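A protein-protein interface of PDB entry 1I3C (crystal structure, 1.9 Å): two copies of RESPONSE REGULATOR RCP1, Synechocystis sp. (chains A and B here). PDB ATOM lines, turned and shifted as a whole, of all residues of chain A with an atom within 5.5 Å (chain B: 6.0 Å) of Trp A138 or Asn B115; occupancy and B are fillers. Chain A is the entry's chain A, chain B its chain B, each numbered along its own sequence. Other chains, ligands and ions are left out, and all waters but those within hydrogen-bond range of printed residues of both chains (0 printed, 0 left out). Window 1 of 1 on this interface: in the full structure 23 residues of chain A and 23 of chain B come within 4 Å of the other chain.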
ATOM      1  N   LEU A  64      14.858 -11.964 -21.585  1.00  0.00           N
ATOM      2  CA  LEU A  64      14.740 -13.145 -20.737  1.00  0.00           C
ATOM      3  C   LEU A  64      13.678 -14.079 -21.298  1.00  0.00           C
ATOM      4  O   LEU A  64      12.590 -13.639 -21.668  1.00  0.00           O
ATOM      5  CB  LEU A  64      14.347 -12.733 -19.316  1.00  0.00           C
ATOM      6  CG  LEU A  64      14.185 -13.857 -18.289  1.00  0.00           C
ATOM      7  CD1 LEU A  64      15.534 -14.542 -18.052  1.00  0.00           C
ATOM      8  CD2 LEU A  64      13.649 -13.280 -16.985  1.00  0.00           C
ATOM      9  N   PRO A  93      19.217 -14.968 -22.235  1.00  0.00           N
ATOM     10  CA  PRO A  93      19.105 -15.913 -21.122  1.00  0.00           C
ATOM     11  C   PRO A  93      17.832 -16.753 -21.210  1.00  0.00           C
ATOM     12  O   PRO A  93      16.741 -16.228 -21.446  1.00  0.00           O
ATOM     13  CB  PRO A  93      19.104 -15.003 -19.897  1.00  0.00           C
ATOM     14  CG  PRO A  93      19.980 -13.870 -20.335  1.00  0.00           C
ATOM     15  CD  PRO A  93      19.479 -13.605 -21.739  1.00  0.00           C
ATOM     16  N   VAL A  95      15.600 -19.576 -19.104  1.00  0.00           N
ATOM     17  CA  VAL A  95      15.347 -20.245 -17.842  1.00  0.00           C
ATOM     18  C   VAL A  95      14.312 -21.318 -18.113  1.00  0.00           C
ATOM     19  O   VAL A  95      13.157 -21.004 -18.397  1.00  0.00           O
ATOM     20  CB  VAL A  95      14.771 -19.275 -16.783  1.00  0.00           C
ATOM     21  CG1 VAL A  95      14.407 -20.043 -15.511  1.00  0.00           C
ATOM     22  CG2 VAL A  95      15.778 -18.181 -16.478  1.00  0.00           C
ATOM     23  N   TYR A 110      21.429 -28.470 -19.818  1.00  0.00           N
ATOM     24  CA  TYR A 110      22.615 -27.696 -19.515  1.00  0.00           C
ATOM     25  C   TYR A 110      23.654 -27.882 -20.615  1.00  0.00           C
ATOM     26  O   TYR A 110      24.420 -26.969 -20.907  1.00  0.00           O
ATOM     27  CB  TYR A 110      23.187 -28.095 -18.154  1.00  0.00           C
ATOM     28  CG  TYR A 110      22.463 -27.439 -17.003  1.00  0.00           C
ATOM     29  CD1 TYR A 110      21.572 -28.158 -16.204  1.00  0.00           C
ATOM     30  CD2 TYR A 110      22.669 -26.088 -16.712  1.00  0.00           C
ATOM     31  CE1 TYR A 110      20.909 -27.544 -15.137  1.00  0.00           C
ATOM     32  CE2 TYR A 110      22.013 -25.467 -15.658  1.00  0.00           C
ATOM     33  CZ  TYR A 110      21.139 -26.195 -14.872  1.00  0.00           C
ATOM     34  OH  TYR A 110      20.509 -25.575 -13.813  1.00  0.00           O
ATOM     35  N   VAL A 114      21.552 -24.153 -21.522  1.00  0.00           N
ATOM     36  CA  VAL A 114      20.429 -23.458 -20.893  1.00  0.00           C
ATOM     37  C   VAL A 114      21.093 -22.681 -19.751  1.00  0.00           C
ATOM     38  O   VAL A 114      22.061 -23.166 -19.153  1.00  0.00           O
ATOM     39  CB  VAL A 114      19.386 -24.452 -20.312  1.00  0.00           C
ATOM     40  CG1 VAL A 114      19.921 -25.100 -19.043  1.00  0.00           C
ATOM     41  CG2 VAL A 114      18.074 -23.729 -20.037  1.00  0.00           C
ATOM     42  N   ASN A 115      20.610 -21.480 -19.452  1.00  0.00           N
ATOM     43  CA  ASN A 115      21.216 -20.705 -18.377  1.00  0.00           C
ATOM     44  C   ASN A 115      20.918 -21.336 -17.020  1.00  0.00           C
ATOM     45  O   ASN A 115      21.755 -21.320 -16.123  1.00  0.00           O
ATOM     46  CB  ASN A 115      20.747 -19.254 -18.439  1.00  0.00           C
ATOM     47  CG  ASN A 115      21.127 -18.591 -19.747  1.00  0.00           C
ATOM     48  OD1 ASN A 115      20.695 -19.024 -20.811  1.00  0.00           O
ATOM     49  ND2 ASN A 115      21.949 -17.542 -19.678  1.00  0.00           N
ATOM     50  N   CYS A 116      19.725 -21.896 -16.867  1.00  0.00           N
ATOM     51  CA  CYS A 116      19.385 -22.584 -15.628  1.00  0.00           C
ATOM     52  C   CYS A 116      18.151 -23.443 -15.817  1.00  0.00           C
ATOM     53  O   CYS A 116      17.325 -23.191 -16.694  1.00  0.00           O
ATOM     54  CB  CYS A 116      19.197 -21.607 -14.460  1.00  0.00           C
ATOM     55  SG  CYS A 116      17.779 -20.540 -14.547  1.00  0.00           S
ATOM     56  N   GLY A 133      11.248 -15.939  -7.117  1.00  0.00           N
ATOM     57  CA  GLY A 133      12.694 -16.057  -7.161  1.00  0.00           C
ATOM     58  C   GLY A 133      13.215 -15.723  -8.547  1.00  0.00           C
ATOM     59  O   GLY A 133      14.251 -15.072  -8.691  1.00  0.00           O
ATOM     60  N   ILE A 134      12.502 -16.176  -9.575  1.00  0.00           N
ATOM     61  CA  ILE A 134      12.895 -15.889 -10.951  1.00  0.00           C
ATOM     62  C   ILE A 134      12.862 -14.378 -11.153  1.00  0.00           C
ATOM     63  O   ILE A 134      13.765 -13.798 -11.762  1.00  0.00           O
ATOM     64  CB  ILE A 134      11.924 -16.551 -11.972  1.00  0.00           C
ATOM     65  CG1 ILE A 134      12.096 -18.072 -11.938  1.00  0.00           C
ATOM     66  CG2 ILE A 134      12.187 -16.010 -13.387  1.00  0.00           C
ATOM     67  CD1 ILE A 134      11.104 -18.826 -12.808  1.00  0.00           C
ATOM     68  N   GLU A 135      11.819 -13.745 -10.625  1.00  0.00           N
ATOM     69  CA  GLU A 135      11.654 -12.300 -10.758  1.00  0.00           C
ATOM     70  C   GLU A 135      12.738 -11.504 -10.041  1.00  0.00           C
ATOM     71  O   GLU A 135      13.379 -10.640 -10.641  1.00  0.00           O
ATOM     72  CB  GLU A 135      10.276 -11.879 -10.227  1.00  0.00           C
ATOM     73  CG  GLU A 135       9.854 -10.432 -10.541  1.00  0.00           C
ATOM     74  CD  GLU A 135      10.567  -9.384  -9.703  1.00  0.00           C
ATOM     75  OE1 GLU A 135      10.755  -9.611  -8.488  1.00  0.00           O
ATOM     76  OE2 GLU A 135      10.922  -8.318 -10.258  1.00  0.00           O
ATOM     77  N   SER A 136      12.961 -11.799  -8.764  1.00  0.00           N
ATOM     78  CA  SER A 136      13.948 -11.042  -8.008  1.00  0.00           C
ATOM     79  C   SER A 136      15.378 -11.238  -8.485  1.00  0.00           C
ATOM     80  O   SER A 136      16.160 -10.287  -8.483  1.00  0.00           O
ATOM     81  CB  SER A 136      13.843 -11.355  -6.507  1.00  0.00           C
ATOM     82  OG  SER A 136      14.194 -12.689  -6.211  1.00  0.00           O
ATOM     83  N   PHE A 137      15.724 -12.450  -8.911  1.00  0.00           N
ATOM     84  CA  PHE A 137      17.085 -12.691  -9.370  1.00  0.00           C
ATOM     85  C   PHE A 137      17.340 -12.196 -10.788  1.00  0.00           C
ATOM     86  O   PHE A 137      18.185 -11.328 -11.001  1.00  0.00           O
ATOM     87  CB  PHE A 137      17.452 -14.182  -9.290  1.00  0.00           C
ATOM     88  CG  PHE A 137      18.901 -14.449  -9.575  1.00  0.00           C
ATOM     89  CD1 PHE A 137      19.886 -13.990  -8.700  1.00  0.00           C
ATOM     90  CD2 PHE A 137      19.294 -15.098 -10.745  1.00  0.00           C
ATOM     91  CE1 PHE A 137      21.242 -14.169  -8.984  1.00  0.00           C
ATOM     92  CE2 PHE A 137      20.654 -15.281 -11.041  1.00  0.00           C
ATOM     93  CZ  PHE A 137      21.626 -14.815 -10.158  1.00  0.00           C
ATOM     94  N   TRP A 138      16.597 -12.737 -11.751  1.00  0.00           N
ATOM     95  CA  TRP A 138      16.777 -12.373 -13.155  1.00  0.00           C
ATOM     96  C   TRP A 138      16.296 -10.998 -13.589  1.00  0.00           C
ATOM     97  O   TRP A 138      16.929 -10.361 -14.434  1.00  0.00           O
ATOM     98  CB  TRP A 138      16.132 -13.427 -14.057  1.00  0.00           C
ATOM     99  CG  TRP A 138      16.792 -14.759 -13.948  1.00  0.00           C
ATOM    100  CD1 TRP A 138      16.437 -15.789 -13.128  1.00  0.00           C
ATOM    101  CD2 TRP A 138      17.970 -15.184 -14.641  1.00  0.00           C
ATOM    102  NE1 TRP A 138      17.321 -16.831 -13.267  1.00  0.00           N
ATOM    103  CE2 TRP A 138      18.274 -16.485 -14.189  1.00  0.00           C
ATOM    104  CE3 TRP A 138      18.802 -14.587 -15.601  1.00  0.00           C
ATOM    105  CZ2 TRP A 138      19.376 -17.207 -14.664  1.00  0.00           C
ATOM    106  CZ3 TRP A 138      19.899 -15.303 -16.074  1.00  0.00           C
ATOM    107  CH2 TRP A 138      20.174 -16.600 -15.604  1.00  0.00           C
ATOM    108  N   LEU A 139      15.187 -10.534 -13.024  1.00  0.00           N
ATOM    109  CA  LEU A 139      14.654  -9.238 -13.416  1.00  0.00           C
ATOM    110  C   LEU A 139      15.166  -8.068 -12.569  1.00  0.00           C
ATOM    111  O   LEU A 139      15.256  -6.948 -13.064  1.00  0.00           O
ATOM    112  CB  LEU A 139      13.121  -9.283 -13.393  1.00  0.00           C
ATOM    113  CG  LEU A 139      12.384  -8.234 -14.222  1.00  0.00           C
ATOM    114  CD1 LEU A 139      12.918  -8.250 -15.656  1.00  0.00           C
ATOM    115  CD2 LEU A 139      10.888  -8.526 -14.203  1.00  0.00           C
ATOM    116  N   GLU A 140      15.521  -8.328 -11.309  1.00  0.00           N
ATOM    117  CA  GLU A 140      16.008  -7.264 -10.427  1.00  0.00           C
ATOM    118  C   GLU A 140      17.497  -7.280 -10.082  1.00  0.00           C
ATOM    119  O   GLU A 140      18.065  -6.237  -9.763  1.00  0.00           O
ATOM    120  CB  GLU A 140      15.242  -7.263  -9.100  1.00  0.00           C
ATOM    121  CG  GLU A 140      13.742  -7.075  -9.196  1.00  0.00           C
ATOM    122  CD  GLU A 140      13.110  -6.849  -7.831  1.00  0.00           C
ATOM    123  OE1 GLU A 140      13.224  -5.719  -7.304  1.00  0.00           O
ATOM    124  OE2 GLU A 140      12.515  -7.803  -7.278  1.00  0.00           O
ATOM    125  N   THR A 141      18.129  -8.448 -10.135  1.00  0.00           N
ATOM    126  CA  THR A 141      19.540  -8.560  -9.761  1.00  0.00           C
ATOM    127  C   THR A 141      20.507  -8.736 -10.920  1.00  0.00           C
ATOM    128  O   THR A 141      21.573  -8.119 -10.955  1.00  0.00           O
ATOM    129  CB  THR A 141      19.736  -9.736  -8.790  1.00  0.00           C
ATOM    130  OG1 THR A 141      18.768  -9.641  -7.741  1.00  0.00           O
ATOM    131  CG2 THR A 141      21.133  -9.715  -8.175  1.00  0.00           C
ATOM    132  N   VAL A 142      20.137  -9.591 -11.864  1.00  0.00           N
ATOM    133  CA  VAL A 142      20.988  -9.863 -13.012  1.00  0.00           C
ATOM    134  C   VAL A 142      21.007  -8.722 -14.018  1.00  0.00           C
ATOM    135  O   VAL A 142      20.034  -7.985 -14.161  1.00  0.00           O
ATOM    136  CB  VAL A 142      20.522 -11.153 -13.746  1.00  0.00           C
ATOM    137  CG1 VAL A 142      21.293 -11.336 -15.056  1.00  0.00           C
ATOM    138  CG2 VAL A 142      20.726 -12.353 -12.848  1.00  0.00           C
ATOM    139  N   LEU A 144      20.781  -8.207 -17.542  1.00  0.00           N
ATOM    140  CA  LEU A 144      20.373  -8.909 -18.753  1.00  0.00           C
ATOM    141  C   LEU A 144      21.008  -8.225 -19.959  1.00  0.00           C
ATOM    142  O   LEU A 144      21.122  -6.998 -20.001  1.00  0.00           O
ATOM    143  CB  LEU A 144      18.845  -8.889 -18.888  1.00  0.00           C
ATOM    144  CG  LEU A 144      18.036  -9.525 -17.747  1.00  0.00           C
ATOM    145  CD1 LEU A 144      16.563  -9.187 -17.922  1.00  0.00           C
ATOM    146  CD2 LEU A 144      18.245 -11.034 -17.726  1.00  0.00           C
ATOM    147  N   LEU B  80      36.444 -17.560 -18.476  1.00  0.00           N
ATOM    148  CA  LEU B  80      35.064 -17.829 -18.876  1.00  0.00           C
ATOM    149  C   LEU B  80      35.015 -18.578 -20.209  1.00  0.00           C
ATOM    150  O   LEU B  80      34.376 -19.631 -20.326  1.00  0.00           O
ATOM    151  CB  LEU B  80      34.286 -16.512 -18.997  1.00  0.00           C
ATOM    152  CG  LEU B  80      32.861 -16.595 -19.563  1.00  0.00           C
ATOM    153  CD1 LEU B  80      32.011 -17.525 -18.709  1.00  0.00           C
ATOM    154  CD2 LEU B  80      32.248 -15.196 -19.621  1.00  0.00           C
ATOM    155  N   LYS B  84      33.711 -22.505 -20.658  1.00  0.00           N
ATOM    156  CA  LYS B  84      32.539 -22.780 -21.478  1.00  0.00           C
ATOM    157  C   LYS B  84      32.754 -23.517 -22.795  1.00  0.00           C
ATOM    158  O   LYS B  84      31.786 -23.953 -23.416  1.00  0.00           O
ATOM    159  CB  LYS B  84      31.775 -21.479 -21.720  1.00  0.00           C
ATOM    160  CG  LYS B  84      31.047 -20.994 -20.469  1.00  0.00           C
ATOM    161  CD  LYS B  84      29.964 -21.988 -20.055  1.00  0.00           C
ATOM    162  CE  LYS B  84      29.345 -21.641 -18.704  1.00  0.00           C
ATOM    163  NZ  LYS B  84      28.238 -22.583 -18.345  1.00  0.00           N
ATOM    164  N   LYS B  90      31.891 -27.111 -19.390  1.00  0.00           N
ATOM    165  CA  LYS B  90      30.827 -26.232 -19.881  1.00  0.00           C
ATOM    166  C   LYS B  90      29.445 -26.388 -19.245  1.00  0.00           C
ATOM    167  O   LYS B  90      28.611 -25.485 -19.323  1.00  0.00           O
ATOM    168  CB  LYS B  90      30.715 -26.368 -21.403  1.00  0.00           C
ATOM    169  CG  LYS B  90      30.421 -27.773 -21.890  1.00  0.00           C
ATOM    170  CD  LYS B  90      30.655 -27.895 -23.388  1.00  0.00           C
ATOM    171  CE  LYS B  90      29.655 -27.089 -24.188  1.00  0.00           C
ATOM    172  NZ  LYS B  90      28.280 -27.646 -24.069  1.00  0.00           N
ATOM    173  N   ARG B  91      29.208 -27.528 -18.612  1.00  0.00           N
ATOM    174  CA  ARG B  91      27.933 -27.817 -17.971  1.00  0.00           C
ATOM    175  C   ARG B  91      27.773 -27.080 -16.634  1.00  0.00           C
ATOM    176  O   ARG B  91      26.656 -26.838 -16.177  1.00  0.00           O
ATOM    177  CB  ARG B  91      27.832 -29.326 -17.740  1.00  0.00           C
ATOM    178  CG  ARG B  91      26.580 -29.798 -17.051  1.00  0.00           C
ATOM    179  CD  ARG B  91      26.731 -31.263 -16.653  1.00  0.00           C
ATOM    180  NE  ARG B  91      27.061 -32.110 -17.797  1.00  0.00           N
ATOM    181  CZ  ARG B  91      27.229 -33.426 -17.728  1.00  0.00           C
ATOM    182  NH1 ARG B  91      27.100 -34.057 -16.568  1.00  0.00           N
ATOM    183  NH2 ARG B  91      27.515 -34.117 -18.823  1.00  0.00           N
ATOM    184  N   ILE B  92      28.895 -26.727 -16.016  1.00  0.00           N
ATOM    185  CA  ILE B  92      28.880 -26.046 -14.723  1.00  0.00           C
ATOM    186  C   ILE B  92      28.410 -24.598 -14.826  1.00  0.00           C
ATOM    187  O   ILE B  92      28.954 -23.808 -15.599  1.00  0.00           O
ATOM    188  CB  ILE B  92      30.289 -26.062 -14.078  1.00  0.00           C
ATOM    189  CG1 ILE B  92      30.839 -27.491 -14.057  1.00  0.00           C
ATOM    190  CG2 ILE B  92      30.223 -25.516 -12.659  1.00  0.00           C
ATOM    191  CD1 ILE B  92      32.312 -27.570 -13.676  1.00  0.00           C
ATOM    192  N   PRO B  93      27.383 -24.229 -14.046  1.00  0.00           N
ATOM    193  CA  PRO B  93      26.886 -22.853 -14.096  1.00  0.00           C
ATOM    194  C   PRO B  93      27.939 -21.851 -13.646  1.00  0.00           C
ATOM    195  O   PRO B  93      28.587 -22.039 -12.613  1.00  0.00           O
ATOM    196  CB  PRO B  93      25.687 -22.885 -13.147  1.00  0.00           C
ATOM    197  CG  PRO B  93      25.182 -24.296 -13.308  1.00  0.00           C
ATOM    198  CD  PRO B  93      26.474 -25.083 -13.258  1.00  0.00           C
ATOM    199  N   VAL B  94      28.111 -20.795 -14.433  1.00  0.00           N
ATOM    200  CA  VAL B  94      29.063 -19.744 -14.114  1.00  0.00           C
ATOM    201  C   VAL B  94      28.328 -18.431 -13.886  1.00  0.00           C
ATOM    202  O   VAL B  94      27.579 -17.960 -14.751  1.00  0.00           O
ATOM    203  CB  VAL B  94      30.089 -19.533 -15.247  1.00  0.00           C
ATOM    204  CG1 VAL B  94      30.972 -18.324 -14.930  1.00  0.00           C
ATOM    205  CG2 VAL B  94      30.952 -20.778 -15.405  1.00  0.00           C
ATOM    206  N   VAL B  95      28.530 -17.860 -12.706  1.00  0.00           N
ATOM    207  CA  VAL B  95      27.928 -16.586 -12.349  1.00  0.00           C
ATOM    208  C   VAL B  95      29.039 -15.541 -12.345  1.00  0.00           C
ATOM    209  O   VAL B  95      29.944 -15.596 -11.516  1.00  0.00           O
ATOM    210  CB  VAL B  95      27.295 -16.619 -10.930  1.00  0.00           C
ATOM    211  CG1 VAL B  95      26.806 -15.218 -10.544  1.00  0.00           C
ATOM    212  CG2 VAL B  95      26.136 -17.608 -10.892  1.00  0.00           C
ATOM    213  N   TYR B 110      27.759 -12.994 -22.396  1.00  0.00           N
ATOM    214  CA  TYR B 110      26.640 -13.896 -22.635  1.00  0.00           C
ATOM    215  C   TYR B 110      26.900 -14.687 -23.918  1.00  0.00           C
ATOM    216  O   TYR B 110      26.447 -15.821 -24.058  1.00  0.00           O
ATOM    217  CB  TYR B 110      25.314 -13.131 -22.724  1.00  0.00           C
ATOM    218  CG  TYR B 110      24.709 -12.814 -21.365  1.00  0.00           C
ATOM    219  CD1 TYR B 110      24.780 -11.528 -20.825  1.00  0.00           C
ATOM    220  CD2 TYR B 110      24.088 -13.812 -20.610  1.00  0.00           C
ATOM    221  CE1 TYR B 110      24.248 -11.244 -19.564  1.00  0.00           C
ATOM    222  CE2 TYR B 110      23.548 -13.540 -19.342  1.00  0.00           C
ATOM    223  CZ  TYR B 110      23.633 -12.254 -18.828  1.00  0.00           C
ATOM    224  OH  TYR B 110      23.109 -11.983 -17.581  1.00  0.00           O
ATOM    225  N   HIS B 113      28.588 -17.718 -23.386  1.00  0.00           N
ATOM    226  CA  HIS B 113      27.702 -18.593 -22.620  1.00  0.00           C
ATOM    227  C   HIS B 113      27.730 -18.511 -21.092  1.00  0.00           C
ATOM    228  O   HIS B 113      27.432 -19.491 -20.412  1.00  0.00           O
ATOM    229  CB  HIS B 113      27.877 -20.053 -23.062  1.00  0.00           C
ATOM    230  CG  HIS B 113      27.274 -20.346 -24.401  1.00  0.00           C
ATOM    231  ND1 HIS B 113      28.030 -20.682 -25.503  1.00  0.00           N
ATOM    232  CD2 HIS B 113      25.986 -20.323 -24.822  1.00  0.00           C
ATOM    233  CE1 HIS B 113      27.236 -20.852 -26.544  1.00  0.00           C
ATOM    234  NE2 HIS B 113      25.990 -20.641 -26.159  1.00  0.00           N
ATOM    235  N   VAL B 114      28.073 -17.348 -20.548  1.00  0.00           N
ATOM    236  CA  VAL B 114      28.062 -17.191 -19.098  1.00  0.00           C
ATOM    237  C   VAL B 114      26.584 -17.390 -18.714  1.00  0.00           C
ATOM    238  O   VAL B 114      25.693 -16.970 -19.458  1.00  0.00           O
ATOM    239  CB  VAL B 114      28.554 -15.769 -18.687  1.00  0.00           C
ATOM    240  CG1 VAL B 114      27.516 -14.716 -19.062  1.00  0.00           C
ATOM    241  CG2 VAL B 114      28.859 -15.729 -17.200  1.00  0.00           C
ATOM    242  N   ASN B 115      26.306 -18.039 -17.587  1.00  0.00           N
ATOM    243  CA  ASN B 115      24.908 -18.268 -17.204  1.00  0.00           C
ATOM    244  C   ASN B 115      24.195 -16.977 -16.816  1.00  0.00           C
ATOM    245  O   ASN B 115      23.025 -16.775 -17.144  1.00  0.00           O
ATOM    246  CB  ASN B 115      24.822 -19.290 -16.075  1.00  0.00           C
ATOM    247  CG  ASN B 115      25.380 -20.636 -16.480  1.00  0.00           C
ATOM    248  OD1 ASN B 115      26.582 -20.775 -16.707  1.00  0.00           O
ATOM    249  ND2 ASN B 115      24.509 -21.639 -16.577  1.00  0.00           N
ATOM    250  N   CYS B 116      24.898 -16.107 -16.103  1.00  0.00           N
ATOM    251  CA  CYS B 116      24.337 -14.819 -15.738  1.00  0.00           C
ATOM    252  C   CYS B 116      25.471 -13.861 -15.431  1.00  0.00           C
ATOM    253  O   CYS B 116      26.567 -14.270 -15.031  1.00  0.00           O
ATOM    254  CB  CYS B 116      23.369 -14.930 -14.554  1.00  0.00           C
ATOM    255  SG  CYS B 116      24.064 -15.583 -13.051  1.00  0.00           S
ATOM    256  N   TYR B 117      25.197 -12.581 -15.643  1.00  0.00           N
ATOM    257  CA  TYR B 117      26.169 -11.524 -15.436  1.00  0.00           C
ATOM    258  C   TYR B 117      25.656 -10.594 -14.343  1.00  0.00           C
ATOM    259  O   TYR B 117      24.542 -10.080 -14.436  1.00  0.00           O
ATOM    260  CB  TYR B 117      26.334 -10.748 -16.743  1.00  0.00           C
ATOM    261  CG  TYR B 117      27.476  -9.758 -16.785  1.00  0.00           C
ATOM    262  CD1 TYR B 117      28.597 -10.008 -17.573  1.00  0.00           C
ATOM    263  CD2 TYR B 117      27.421  -8.553 -16.077  1.00  0.00           C
ATOM    264  CE1 TYR B 117      29.631  -9.093 -17.667  1.00  0.00           C
ATOM    265  CE2 TYR B 117      28.465  -7.623 -16.162  1.00  0.00           C
ATOM    266  CZ  TYR B 117      29.564  -7.904 -16.963  1.00  0.00           C
ATOM    267  OH  TYR B 117      30.601  -7.006 -17.073  1.00  0.00           O
ATOM    268  N   PHE B 137      19.049 -18.226  -5.095  1.00  0.00           N
ATOM    269  CA  PHE B 137      18.625 -18.703  -6.405  1.00  0.00           C
ATOM    270  C   PHE B 137      19.364 -19.940  -6.901  1.00  0.00           C
ATOM    271  O   PHE B 137      18.743 -20.948  -7.243  1.00  0.00           O
ATOM    272  CB  PHE B 137      18.748 -17.606  -7.466  1.00  0.00           C
ATOM    273  CG  PHE B 137      18.116 -17.984  -8.776  1.00  0.00           C
ATOM    274  CD1 PHE B 137      16.730 -18.062  -8.888  1.00  0.00           C
ATOM    275  CD2 PHE B 137      18.897 -18.361  -9.860  1.00  0.00           C
ATOM    276  CE1 PHE B 137      16.132 -18.520 -10.062  1.00  0.00           C
ATOM    277  CE2 PHE B 137      18.312 -18.818 -11.035  1.00  0.00           C
ATOM    278  CZ  PHE B 137      16.924 -18.900 -11.136  1.00  0.00           C
ATOM    279  N   TRP B 138      20.690 -19.871  -6.936  1.00  0.00           N
ATOM    280  CA  TRP B 138      21.479 -20.986  -7.437  1.00  0.00           C
ATOM    281  C   TRP B 138      21.643 -22.180  -6.506  1.00  0.00           C
ATOM    282  O   TRP B 138      21.824 -23.307  -6.973  1.00  0.00           O
ATOM    283  CB  TRP B 138      22.858 -20.484  -7.886  1.00  0.00           C
ATOM    284  CG  TRP B 138      22.778 -19.602  -9.091  1.00  0.00           C
ATOM    285  CD1 TRP B 138      22.742 -18.233  -9.112  1.00  0.00           C
ATOM    286  CD2 TRP B 138      22.640 -20.027 -10.449  1.00  0.00           C
ATOM    287  NE1 TRP B 138      22.587 -17.784 -10.404  1.00  0.00           N
ATOM    288  CE2 TRP B 138      22.521 -18.865 -11.243  1.00  0.00           C
ATOM    289  CE3 TRP B 138      22.602 -21.282 -11.076  1.00  0.00           C
ATOM    290  CZ2 TRP B 138      22.364 -18.921 -12.634  1.00  0.00           C
ATOM    291  CZ3 TRP B 138      22.447 -21.335 -12.460  1.00  0.00           C
ATOM    292  CH2 TRP B 138      22.330 -20.161 -13.221  1.00  0.00           C
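O of Asn A115 sits at hydrogen-bond distance from ND2 of Asn B115, 2.8 Å away.
The side-chain hydroxyl of Tyr B110 lies within hydrogen-bond range of the backbone NH of Tyr B117 (2.9 Å).
N of Val A142 sits at hydrogen-bond distance from O of Phe A137 (2.8 Å).
The side-chain amide oxygen (OD1) of Asn B115 is in hydrogen-bond range of the backbone NH (N) of Val B94 (2.7 Å).
The side-chain amino group (NZ) of Lys B84 lies within hydrogen-bond range of the side-chain amide oxygen (OD1) of Asn B115 (2.9 Å).
NE1 of Trp B138 is in hydrogen-bond range of SG of Cys B116, at 3.7 Å.
O of Gly A133 is in hydrogen-bond range of OG of Ser A136, 3.4 Å away.
Among the printed residues, merely in contact across the chains: Trp A138 with Phe B137, Phe A137 with Trp B138, Val A142 with Tyr B110, Asn A115 with Trp B138, Trp A138 with Asn B115, Phe A137 with Phe B137, Val A142 with Tyr B117, Cys A116 with Trp B138, Pro A93 with Tyr B110, Trp A138 with Cys B116, Asn A115 with Val B114, Phe A137 with Cys B116, Val A114 with Asn B115, Cys A116 with Phe B137, Gly A133 with Phe B137, Tyr A110 with Arg B91 and Trp A138 with Trp B138.
Of the printed residues of chain A, Phe B137 touches Cys A116 (3.9 Å), Gly A133 (3.9 Å), Phe A137 (3.4 Å) and Trp A138 (3.0 Å).
Printed residues of chain B within 4 Å of Phe A137: Cys B116, Phe B137 and Trp B138.
Of the printed residues of chain A, Tyr B117 touches Val A142.
Of the printed residues of chain A, Trp B138 touches Asn A115 (3.2 Å), Cys A116 (3.7 Å), Phe A137 (3.1 Å) and Trp A138 (3.998 Å).
The nearest printed residue of chain B that does not touch Trp A138 is Tyr B110 (4.9 Å).
The nearest residue of chain A that does not touch Asn B115 is Tyr A110 (4.7 Å).
The nearest printed residue of chain B that does not touch Val A114 is Lys B84 (6.3 Å).
Of the 16 printed residues of chain B, 8 touch a printed residue of chain A.
Printed residues of chain A that touch a printed residue of chain B: Pro A93, Tyr A110, Val A114, Asn A115, Cys A116, Gly A133, Phe A137, Trp A138 and Val A142.
Among the printed residues, 18 pairs touch across the chains.
Among the printed residues, no Asp or Glu carboxylate lies within 4 Å of a Lys or Arg side-chain nitrogen of the other chain.
Pro A93 touches Tyr B110, but with the chains exchanged Tyr A110 does not touch Pro B93 (4.1 Å).
Asn B115 touches its own counterpart, Asn A115.
Phe A137 touches its own counterpart, Phe B137.
Trp B138 touches its own counterpart, Trp A138.
8 positions are printed for both chains.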
